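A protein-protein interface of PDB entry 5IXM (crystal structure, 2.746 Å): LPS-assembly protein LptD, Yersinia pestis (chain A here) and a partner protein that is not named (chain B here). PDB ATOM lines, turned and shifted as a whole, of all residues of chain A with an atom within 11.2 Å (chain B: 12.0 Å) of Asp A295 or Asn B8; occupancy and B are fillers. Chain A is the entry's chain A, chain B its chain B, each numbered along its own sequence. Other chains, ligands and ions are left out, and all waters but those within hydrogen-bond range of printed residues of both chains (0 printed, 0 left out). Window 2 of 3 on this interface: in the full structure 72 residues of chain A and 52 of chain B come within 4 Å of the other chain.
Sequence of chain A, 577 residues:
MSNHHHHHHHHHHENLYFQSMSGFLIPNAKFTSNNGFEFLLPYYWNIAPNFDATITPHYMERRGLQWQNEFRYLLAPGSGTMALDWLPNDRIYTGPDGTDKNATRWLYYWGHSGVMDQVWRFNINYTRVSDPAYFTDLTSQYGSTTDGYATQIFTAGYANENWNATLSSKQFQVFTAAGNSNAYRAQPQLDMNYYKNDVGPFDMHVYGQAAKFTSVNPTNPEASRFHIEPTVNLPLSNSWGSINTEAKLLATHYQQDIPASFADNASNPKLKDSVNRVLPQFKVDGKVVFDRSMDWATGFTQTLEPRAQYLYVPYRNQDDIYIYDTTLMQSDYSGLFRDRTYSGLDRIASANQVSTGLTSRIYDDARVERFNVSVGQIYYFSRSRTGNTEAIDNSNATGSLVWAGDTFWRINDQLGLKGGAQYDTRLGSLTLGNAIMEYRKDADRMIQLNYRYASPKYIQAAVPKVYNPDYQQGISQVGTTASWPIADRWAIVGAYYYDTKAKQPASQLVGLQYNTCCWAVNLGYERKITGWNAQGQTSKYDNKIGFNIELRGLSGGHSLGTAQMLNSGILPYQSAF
The backbone NH of Asp A291 sits at hydrogen-bond distance from the backbone carbonyl oxygen of Gly B11 (3.0 Å).
OD1 of Asp A295 sits close to OD1 of Asn B8 (2.7 Å).
The backbone carbonyl oxygen (O) of Gln A302 is in hydrogen-bond range of the guanidinium group (NH1) of Arg B10, at 3.0 Å.
The guanidinium group (NE) of Arg A292 sits close to the guanidinium group (NH2) of Arg B10, 3.4 Å away.
N of Phe A290 lies within hydrogen-bond range of O of Leu A304 (2.9 Å).
NH1 of Arg A292 is in salt-bridge range of OD2 of Asp A295, 3.9 Å away.
The side-chain amide oxygen (OE1) of Gln A302 lies within hydrogen-bond range of the guanidinium group (NH2) of Arg A292, 2.7 Å away.
Among the printed residues, merely in contact across the chains: Phe A290 with Gly B11, Phe A290 with Thr B12, Asp A291 with Arg B10, Arg A292 with Asn B8, Ser A293 with Asn B8 and Leu A304 with Arg B10.
Of the printed residues of chain B, Phe A290 touches Gly B11 (3.5 Å) and Thr B12 (3.6 Å).
Of the printed residues of chain B, Asp A291 touches Arg B10 and Gly B11.
Of chain B, only Asn B8 (3.5 Å) and Arg B10 (3.3 Å) come within 4 Å of Arg A292.
No residue of chain B comes within 4 Å of Met A294.
Asp A295 touches just one residue of chain B: Asn B8 (2.7 Å).
No residue of chain B comes within 4 Å of Trp A296.
No residue of chain B comes within 4 Å of Ala A297.
No residue of chain B comes within 4 Å of Thr A298.
Of the printed residues of chain B, Gln A302 touches Arg B10 (3.0 Å).
Thr A303 touches none of the printed residues of chain B.
Printed residues of chain B within 4 Å of Leu A304: Arg B10 (3.97 Å).
No residue of chain A comes within 4 Å of Phe B7.
Printed residues of chain A within 4 Å of Asn B8: Arg A292, Ser A293 and Asp A295.
No residue of chain A comes within 4 Å of Leu B9.
Of the printed residues of chain A, Thr B12 touches Phe A290.
The nearest residue of chain B that does not touch Asp A295 is Leu B9 (5.9 Å).
Along chain A the printed residues that touch a printed residue of chain B span positions 290 to 304.
Of the 7 printed residues of chain B, 4 touch a printed residue of chain A.
Among the printed residues, 10 pairs touch across the chains.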
ATOM      1  N   PHE A 290     -12.933 -13.317  22.248  1.00  0.00           N
ATOM      2  CA  PHE A 290     -14.175 -13.170  23.003  1.00  0.00           C
ATOM      3  C   PHE A 290     -15.360 -13.447  22.085  1.00  0.00           C
ATOM      4  O   PHE A 290     -15.241 -13.341  20.864  1.00  0.00           O
ATOM      5  CB  PHE A 290     -14.324 -11.765  23.596  1.00  0.00           C
ATOM      6  CG  PHE A 290     -13.206 -11.350  24.509  1.00  0.00           C
ATOM      7  CD1 PHE A 290     -12.100 -10.679  24.015  1.00  0.00           C
ATOM      8  CD2 PHE A 290     -13.282 -11.594  25.871  1.00  0.00           C
ATOM      9  CE1 PHE A 290     -11.077 -10.281  24.859  1.00  0.00           C
ATOM     10  CE2 PHE A 290     -12.264 -11.198  26.719  1.00  0.00           C
ATOM     11  CZ  PHE A 290     -11.159 -10.541  26.213  1.00  0.00           C
ATOM     12  N   ASP A 291     -16.506 -13.784  22.668  1.00  0.00           N
ATOM     13  CA  ASP A 291     -17.738 -13.896  21.893  1.00  0.00           C
ATOM     14  C   ASP A 291     -18.982 -13.698  22.756  1.00  0.00           C
ATOM     15  O   ASP A 291     -18.909 -13.734  23.986  1.00  0.00           O
ATOM     16  CB  ASP A 291     -17.799 -15.250  21.164  1.00  0.00           C
ATOM     17  CG  ASP A 291     -17.817 -16.446  22.112  1.00  0.00           C
ATOM     18  OD1 ASP A 291     -17.983 -16.271  23.337  1.00  0.00           O
ATOM     19  OD2 ASP A 291     -17.671 -17.585  21.615  1.00  0.00           O
ATOM     20  N   ARG A 292     -20.119 -13.483  22.103  1.00  0.00           N
ATOM     21  CA  ARG A 292     -21.378 -13.296  22.816  1.00  0.00           C
ATOM     22  C   ARG A 292     -22.567 -13.527  21.901  1.00  0.00           C
ATOM     23  O   ARG A 292     -22.475 -13.352  20.684  1.00  0.00           O
ATOM     24  CB  ARG A 292     -21.463 -11.892  23.427  1.00  0.00           C
ATOM     25  CG  ARG A 292     -21.608 -10.762  22.419  1.00  0.00           C
ATOM     26  CD  ARG A 292     -21.688  -9.414  23.124  1.00  0.00           C
ATOM     27  NE  ARG A 292     -21.807  -8.300  22.186  1.00  0.00           N
ATOM     28  CZ  ARG A 292     -22.964  -7.798  21.765  1.00  0.00           C
ATOM     29  NH1 ARG A 292     -24.110  -8.311  22.196  1.00  0.00           N
ATOM     30  NH2 ARG A 292     -22.976  -6.782  20.911  1.00  0.00           N
ATOM     31  N   SER A 293     -23.684 -13.924  22.499  1.00  0.00           N
ATOM     32  CA  SER A 293     -24.953 -13.979  21.791  1.00  0.00           C
ATOM     33  C   SER A 293     -25.554 -12.584  21.774  1.00  0.00           C
ATOM     34  O   SER A 293     -25.721 -11.963  22.824  1.00  0.00           O
ATOM     35  CB  SER A 293     -25.912 -14.974  22.449  1.00  0.00           C
ATOM     36  OG  SER A 293     -25.384 -16.289  22.420  1.00  0.00           O
ATOM     37  N   MET A 294     -25.865 -12.091  20.579  1.00  0.00           N
ATOM     38  CA  MET A 294     -26.417 -10.750  20.429  1.00  0.00           C
ATOM     39  C   MET A 294     -27.773 -10.687  21.127  1.00  0.00           C
ATOM     40  O   MET A 294     -28.445 -11.705  21.286  1.00  0.00           O
ATOM     41  CB  MET A 294     -26.517 -10.373  18.952  1.00  0.00           C
ATOM     42  CG  MET A 294     -25.184 -10.503  18.221  1.00  0.00           C
ATOM     43  SD  MET A 294     -25.130  -9.741  16.588  1.00  0.00           S
ATOM     44  CE  MET A 294     -25.431  -8.024  17.002  1.00  0.00           C
ATOM     45  N   ASP A 295     -28.179  -9.487  21.527  1.00  0.00           N
ATOM     46  CA  ASP A 295     -29.298  -9.333  22.451  1.00  0.00           C
ATOM     47  C   ASP A 295     -30.661  -9.465  21.784  1.00  0.00           C
ATOM     48  O   ASP A 295     -31.311 -10.507  21.882  1.00  0.00           O
ATOM     49  CB  ASP A 295     -29.205  -7.972  23.144  1.00  0.00           C
ATOM     50  CG  ASP A 295     -27.866  -7.757  23.820  1.00  0.00           C
ATOM     51  OD1 ASP A 295     -27.399  -8.680  24.515  1.00  0.00           O
ATOM     52  OD2 ASP A 295     -27.277  -6.668  23.648  1.00  0.00           O
ATOM     53  N   TRP A 296     -31.094  -8.401  21.121  1.00  0.00           N
ATOM     54  CA  TRP A 296     -32.376  -8.393  20.429  1.00  0.00           C
ATOM     55  C   TRP A 296     -32.409  -9.404  19.286  1.00  0.00           C
ATOM     56  O   TRP A 296     -33.444 -10.015  19.019  1.00  0.00           O
ATOM     57  CB  TRP A 296     -32.688  -6.977  19.945  1.00  0.00           C
ATOM     58  CG  TRP A 296     -32.795  -6.014  21.092  1.00  0.00           C
ATOM     59  CD1 TRP A 296     -32.849  -6.334  22.421  1.00  0.00           C
ATOM     60  CD2 TRP A 296     -32.828  -4.583  21.025  1.00  0.00           C
ATOM     61  NE1 TRP A 296     -32.935  -5.196  23.181  1.00  0.00           N
ATOM     62  CE2 TRP A 296     -32.921  -4.107  22.352  1.00  0.00           C
ATOM     63  CE3 TRP A 296     -32.798  -3.661  19.977  1.00  0.00           C
ATOM     64  CZ2 TRP A 296     -32.982  -2.747  22.654  1.00  0.00           C
ATOM     65  CZ3 TRP A 296     -32.858  -2.309  20.282  1.00  0.00           C
ATOM     66  CH2 TRP A 296     -32.950  -1.866  21.609  1.00  0.00           C
ATOM     67  N   ALA A 297     -31.278  -9.582  18.612  1.00  0.00           N
ATOM     68  CA  ALA A 297     -31.184 -10.603  17.577  1.00  0.00           C
ATOM     69  C   ALA A 297     -30.695 -11.908  18.196  1.00  0.00           C
ATOM     70  O   ALA A 297     -29.527 -12.033  18.566  1.00  0.00           O
ATOM     71  CB  ALA A 297     -30.256 -10.154  16.460  1.00  0.00           C
ATOM     72  N   THR A 298     -31.600 -12.876  18.308  1.00  0.00           N
ATOM     73  CA  THR A 298     -31.293 -14.147  18.955  1.00  0.00           C
ATOM     74  C   THR A 298     -30.882 -15.201  17.934  1.00  0.00           C
ATOM     75  O   THR A 298     -31.523 -15.354  16.893  1.00  0.00           O
ATOM     76  CB  THR A 298     -32.494 -14.673  19.770  1.00  0.00           C
ATOM     77  OG1 THR A 298     -33.020 -13.619  20.587  1.00  0.00           O
ATOM     78  CG2 THR A 298     -32.072 -15.836  20.660  1.00  0.00           C
ATOM     79  N   GLY A 299     -29.812 -15.925  18.239  1.00  0.00           N
ATOM     80  CA  GLY A 299     -29.316 -16.956  17.349  1.00  0.00           C
ATOM     81  C   GLY A 299     -27.988 -16.546  16.745  1.00  0.00           C
ATOM     82  O   GLY A 299     -27.162 -17.390  16.395  1.00  0.00           O
ATOM     83  N   PHE A 300     -27.785 -15.239  16.630  1.00  0.00           N
ATOM     84  CA  PHE A 300     -26.567 -14.702  16.040  1.00  0.00           C
ATOM     85  C   PHE A 300     -25.472 -14.606  17.091  1.00  0.00           C
ATOM     86  O   PHE A 300     -25.756 -14.461  18.280  1.00  0.00           O
ATOM     87  CB  PHE A 300     -26.827 -13.327  15.413  1.00  0.00           C
ATOM     88  CG  PHE A 300     -27.658 -13.372  14.162  1.00  0.00           C
ATOM     89  CD1 PHE A 300     -29.026 -13.576  14.224  1.00  0.00           C
ATOM     90  CD2 PHE A 300     -27.070 -13.199  12.922  1.00  0.00           C
ATOM     91  CE1 PHE A 300     -29.786 -13.619  13.071  1.00  0.00           C
ATOM     92  CE2 PHE A 300     -27.826 -13.241  11.767  1.00  0.00           C
ATOM     93  CZ  PHE A 300     -29.184 -13.450  11.842  1.00  0.00           C
ATOM     94  N   THR A 301     -24.221 -14.683  16.649  1.00  0.00           N
ATOM     95  CA  THR A 301     -23.093 -14.558  17.565  1.00  0.00           C
ATOM     96  C   THR A 301     -22.105 -13.510  17.083  1.00  0.00           C
ATOM     97  O   THR A 301     -21.691 -13.525  15.927  1.00  0.00           O
ATOM     98  CB  THR A 301     -22.344 -15.895  17.742  1.00  0.00           C
ATOM     99  OG1 THR A 301     -23.230 -16.877  18.291  1.00  0.00           O
ATOM    100  CG2 THR A 301     -21.155 -15.714  18.672  1.00  0.00           C
ATOM    101  N   GLN A 302     -21.733 -12.595  17.969  1.00  0.00           N
ATOM    102  CA  GLN A 302     -20.719 -11.609  17.633  1.00  0.00           C
ATOM    103  C   GLN A 302     -19.429 -11.955  18.365  1.00  0.00           C
ATOM    104  O   GLN A 302     -19.436 -12.216  19.569  1.00  0.00           O
ATOM    105  CB  GLN A 302     -21.188 -10.200  17.985  1.00  0.00           C
ATOM    106  CG  GLN A 302     -20.273  -9.100  17.479  1.00  0.00           C
ATOM    107  CD  GLN A 302     -20.766  -7.714  17.856  1.00  0.00           C
ATOM    108  OE1 GLN A 302     -21.742  -7.567  18.592  1.00  0.00           O
ATOM    109  NE2 GLN A 302     -20.094  -6.689  17.344  1.00  0.00           N
ATOM    110  N   THR A 303     -18.325 -11.973  17.627  1.00  0.00           N
ATOM    111  CA  THR A 303     -17.031 -12.300  18.202  1.00  0.00           C
ATOM    112  C   THR A 303     -16.125 -11.085  18.172  1.00  0.00           C
ATOM    113  O   THR A 303     -16.156 -10.304  17.220  1.00  0.00           O
ATOM    114  CB  THR A 303     -16.345 -13.448  17.447  1.00  0.00           C
ATOM    115  OG1 THR A 303     -15.774 -12.944  16.233  1.00  0.00           O
ATOM    116  CG2 THR A 303     -17.344 -14.542  17.120  1.00  0.00           C
ATOM    117  N   LEU A 304     -15.304 -10.949  19.208  1.00  0.00           N
ATOM    118  CA  LEU A 304     -14.362  -9.844  19.319  1.00  0.00           C
ATOM    119  C   LEU A 304     -12.948 -10.393  19.512  1.00  0.00           C
ATOM    120  O   LEU A 304     -12.661 -11.044  20.509  1.00  0.00           O
ATOM    121  CB  LEU A 304     -14.758  -8.928  20.480  1.00  0.00           C
ATOM    122  CG  LEU A 304     -14.085  -7.560  20.573  1.00  0.00           C
ATOM    123  CD1 LEU A 304     -14.578  -6.647  19.460  1.00  0.00           C
ATOM    124  CD2 LEU A 304     -14.335  -6.941  21.940  1.00  0.00           C
ATOM    125  N   ILE A 362     -19.503 -11.848  12.786  1.00  0.00           N
ATOM    126  CA  ILE A 362     -20.898 -12.146  13.096  1.00  0.00           C
ATOM    127  C   ILE A 362     -21.346 -13.422  12.394  1.00  0.00           C
ATOM    128  O   ILE A 362     -21.317 -13.514  11.170  1.00  0.00           O
ATOM    129  CB  ILE A 362     -21.844 -10.991  12.708  1.00  0.00           C
ATOM    130  CG1 ILE A 362     -21.665  -9.812  13.665  1.00  0.00           C
ATOM    131  CG2 ILE A 362     -23.296 -11.450  12.753  1.00  0.00           C
ATOM    132  CD1 ILE A 362     -22.585  -8.648  13.377  1.00  0.00           C
ATOM    133  N   TYR A 363     -21.755 -14.406  13.186  1.00  0.00           N
ATOM    134  CA  TYR A 363     -22.272 -15.659  12.659  1.00  0.00           C
ATOM    135  C   TYR A 363     -23.784 -15.684  12.849  1.00  0.00           C
ATOM    136  O   TYR A 363     -24.311 -15.027  13.749  1.00  0.00           O
ATOM    137  CB  TYR A 363     -21.624 -16.856  13.359  1.00  0.00           C
ATOM    138  CG  TYR A 363     -20.113 -16.896  13.271  1.00  0.00           C
ATOM    139  CD1 TYR A 363     -19.330 -16.145  14.137  1.00  0.00           C
ATOM    140  CD2 TYR A 363     -19.471 -17.697  12.335  1.00  0.00           C
ATOM    141  CE1 TYR A 363     -17.952 -16.180  14.067  1.00  0.00           C
ATOM    142  CE2 TYR A 363     -18.090 -17.740  12.259  1.00  0.00           C
ATOM    143  CZ  TYR A 363     -17.337 -16.980  13.129  1.00  0.00           C
ATOM    144  OH  TYR A 363     -15.962 -17.016  13.063  1.00  0.00           O
ATOM    145  N   PHE B   7     -24.647 -15.663  28.943  1.00  0.00           N
ATOM    146  CA  PHE B   7     -25.129 -14.590  29.806  1.00  0.00           C
ATOM    147  C   PHE B   7     -24.685 -13.229  29.285  1.00  0.00           C
ATOM    148  O   PHE B   7     -23.896 -12.531  29.925  1.00  0.00           O
ATOM    149  CB  PHE B   7     -24.662 -14.794  31.256  1.00  0.00           C
ATOM    150  CG  PHE B   7     -23.311 -15.440  31.381  1.00  0.00           C
ATOM    151  CD1 PHE B   7     -23.175 -16.818  31.296  1.00  0.00           C
ATOM    152  CD2 PHE B   7     -22.178 -14.674  31.598  1.00  0.00           C
ATOM    153  CE1 PHE B   7     -21.938 -17.417  31.408  1.00  0.00           C
ATOM    154  CE2 PHE B   7     -20.935 -15.269  31.715  1.00  0.00           C
ATOM    155  CZ  PHE B   7     -20.815 -16.643  31.620  1.00  0.00           C
ATOM    156  N   ASN B   8     -25.165 -12.907  28.084  1.00  0.00           N
ATOM    157  CA  ASN B   8     -25.208 -11.547  27.541  1.00  0.00           C
ATOM    158  C   ASN B   8     -23.919 -10.958  26.957  1.00  0.00           C
ATOM    159  O   ASN B   8     -23.810 -10.779  25.745  1.00  0.00           O
ATOM    160  CB  ASN B   8     -25.731 -10.591  28.620  1.00  0.00           C
ATOM    161  CG  ASN B   8     -26.127  -9.235  28.061  1.00  0.00           C
ATOM    162  OD1 ASN B   8     -26.118  -9.022  26.851  1.00  0.00           O
ATOM    163  ND2 ASN B   8     -26.485  -8.313  28.945  1.00  0.00           N
ATOM    164  N   LEU B   9     -22.943 -10.677  27.813  1.00  0.00           N
ATOM    165  CA  LEU B   9     -21.736  -9.971  27.393  1.00  0.00           C
ATOM    166  C   LEU B   9     -20.529 -10.910  27.280  1.00  0.00           C
ATOM    167  O   LEU B   9     -20.642 -12.112  27.521  1.00  0.00           O
ATOM    168  CB  LEU B   9     -21.459  -8.811  28.365  1.00  0.00           C
ATOM    169  CG  LEU B   9     -20.465  -7.690  28.033  1.00  0.00           C
ATOM    170  CD1 LEU B   9     -20.525  -7.321  26.555  1.00  0.00           C
ATOM    171  CD2 LEU B   9     -20.726  -6.470  28.904  1.00  0.00           C
ATOM    172  N   ARG B  10     -19.384 -10.344  26.906  1.00  0.00           N
ATOM    173  CA  ARG B  10     -18.216 -11.080  26.430  1.00  0.00           C
ATOM    174  C   ARG B  10     -17.673 -12.126  27.396  1.00  0.00           C
ATOM    175  O   ARG B  10     -17.384 -11.837  28.559  1.00  0.00           O
ATOM    176  CB  ARG B  10     -17.084 -10.096  26.119  1.00  0.00           C
ATOM    177  CG  ARG B  10     -17.429  -8.983  25.145  1.00  0.00           C
ATOM    178  CD  ARG B  10     -17.943  -9.508  23.822  1.00  0.00           C
ATOM    179  NE  ARG B  10     -18.166  -8.412  22.885  1.00  0.00           N
ATOM    180  CZ  ARG B  10     -18.547  -8.576  21.623  1.00  0.00           C
ATOM    181  NH1 ARG B  10     -18.736  -9.796  21.141  1.00  0.00           N
ATOM    182  NH2 ARG B  10     -18.728  -7.520  20.841  1.00  0.00           N
ATOM    183  N   GLY B  11     -17.555 -13.351  26.895  1.00  0.00           N
ATOM    184  CA  GLY B  11     -16.863 -14.417  27.594  1.00  0.00           C
ATOM    185  C   GLY B  11     -15.874 -15.029  26.620  1.00  0.00           C
ATOM    186  O   GLY B  11     -16.025 -14.881  25.408  1.00  0.00           O
ATOM    187  N   THR B  12     -14.859 -15.714  27.136  1.00  0.00           N
ATOM    188  CA  THR B  12     -13.869 -16.341  26.267  1.00  0.00           C
ATOM    189  C   THR B  12     -14.149 -17.818  26.007  1.00  0.00           C
ATOM    190  O   THR B  12     -14.190 -18.624  26.934  1.00  0.00           O
ATOM    191  CB  THR B  12     -12.449 -16.210  26.855  1.00  0.00           C
ATOM    192  OG1 THR B  12     -12.409 -16.792  28.165  1.00  0.00           O
ATOM    193  CG2 THR B  12     -12.046 -14.751  26.944  1.00  0.00           C
ATOM    194  N   THR B  13     -14.349 -18.159  24.737  1.00  0.00           N
ATOM    195  CA  THR B  13     -14.435 -19.548  24.275  1.00  0.00           C
ATOM    196  C   THR B  13     -14.221 -19.519  22.754  1.00  0.00           C
ATOM    197  O   THR B  13     -13.611 -18.576  22.246  1.00  0.00           O
ATOM    198  CB  THR B  13     -15.773 -20.238  24.652  1.00  0.00           C
ATOM    199  OG1 THR B  13     -16.194 -19.807  25.952  1.00  0.00           O
ATOM    200  CG2 THR B  13     -15.611 -21.763  24.683  1.00  0.00           C
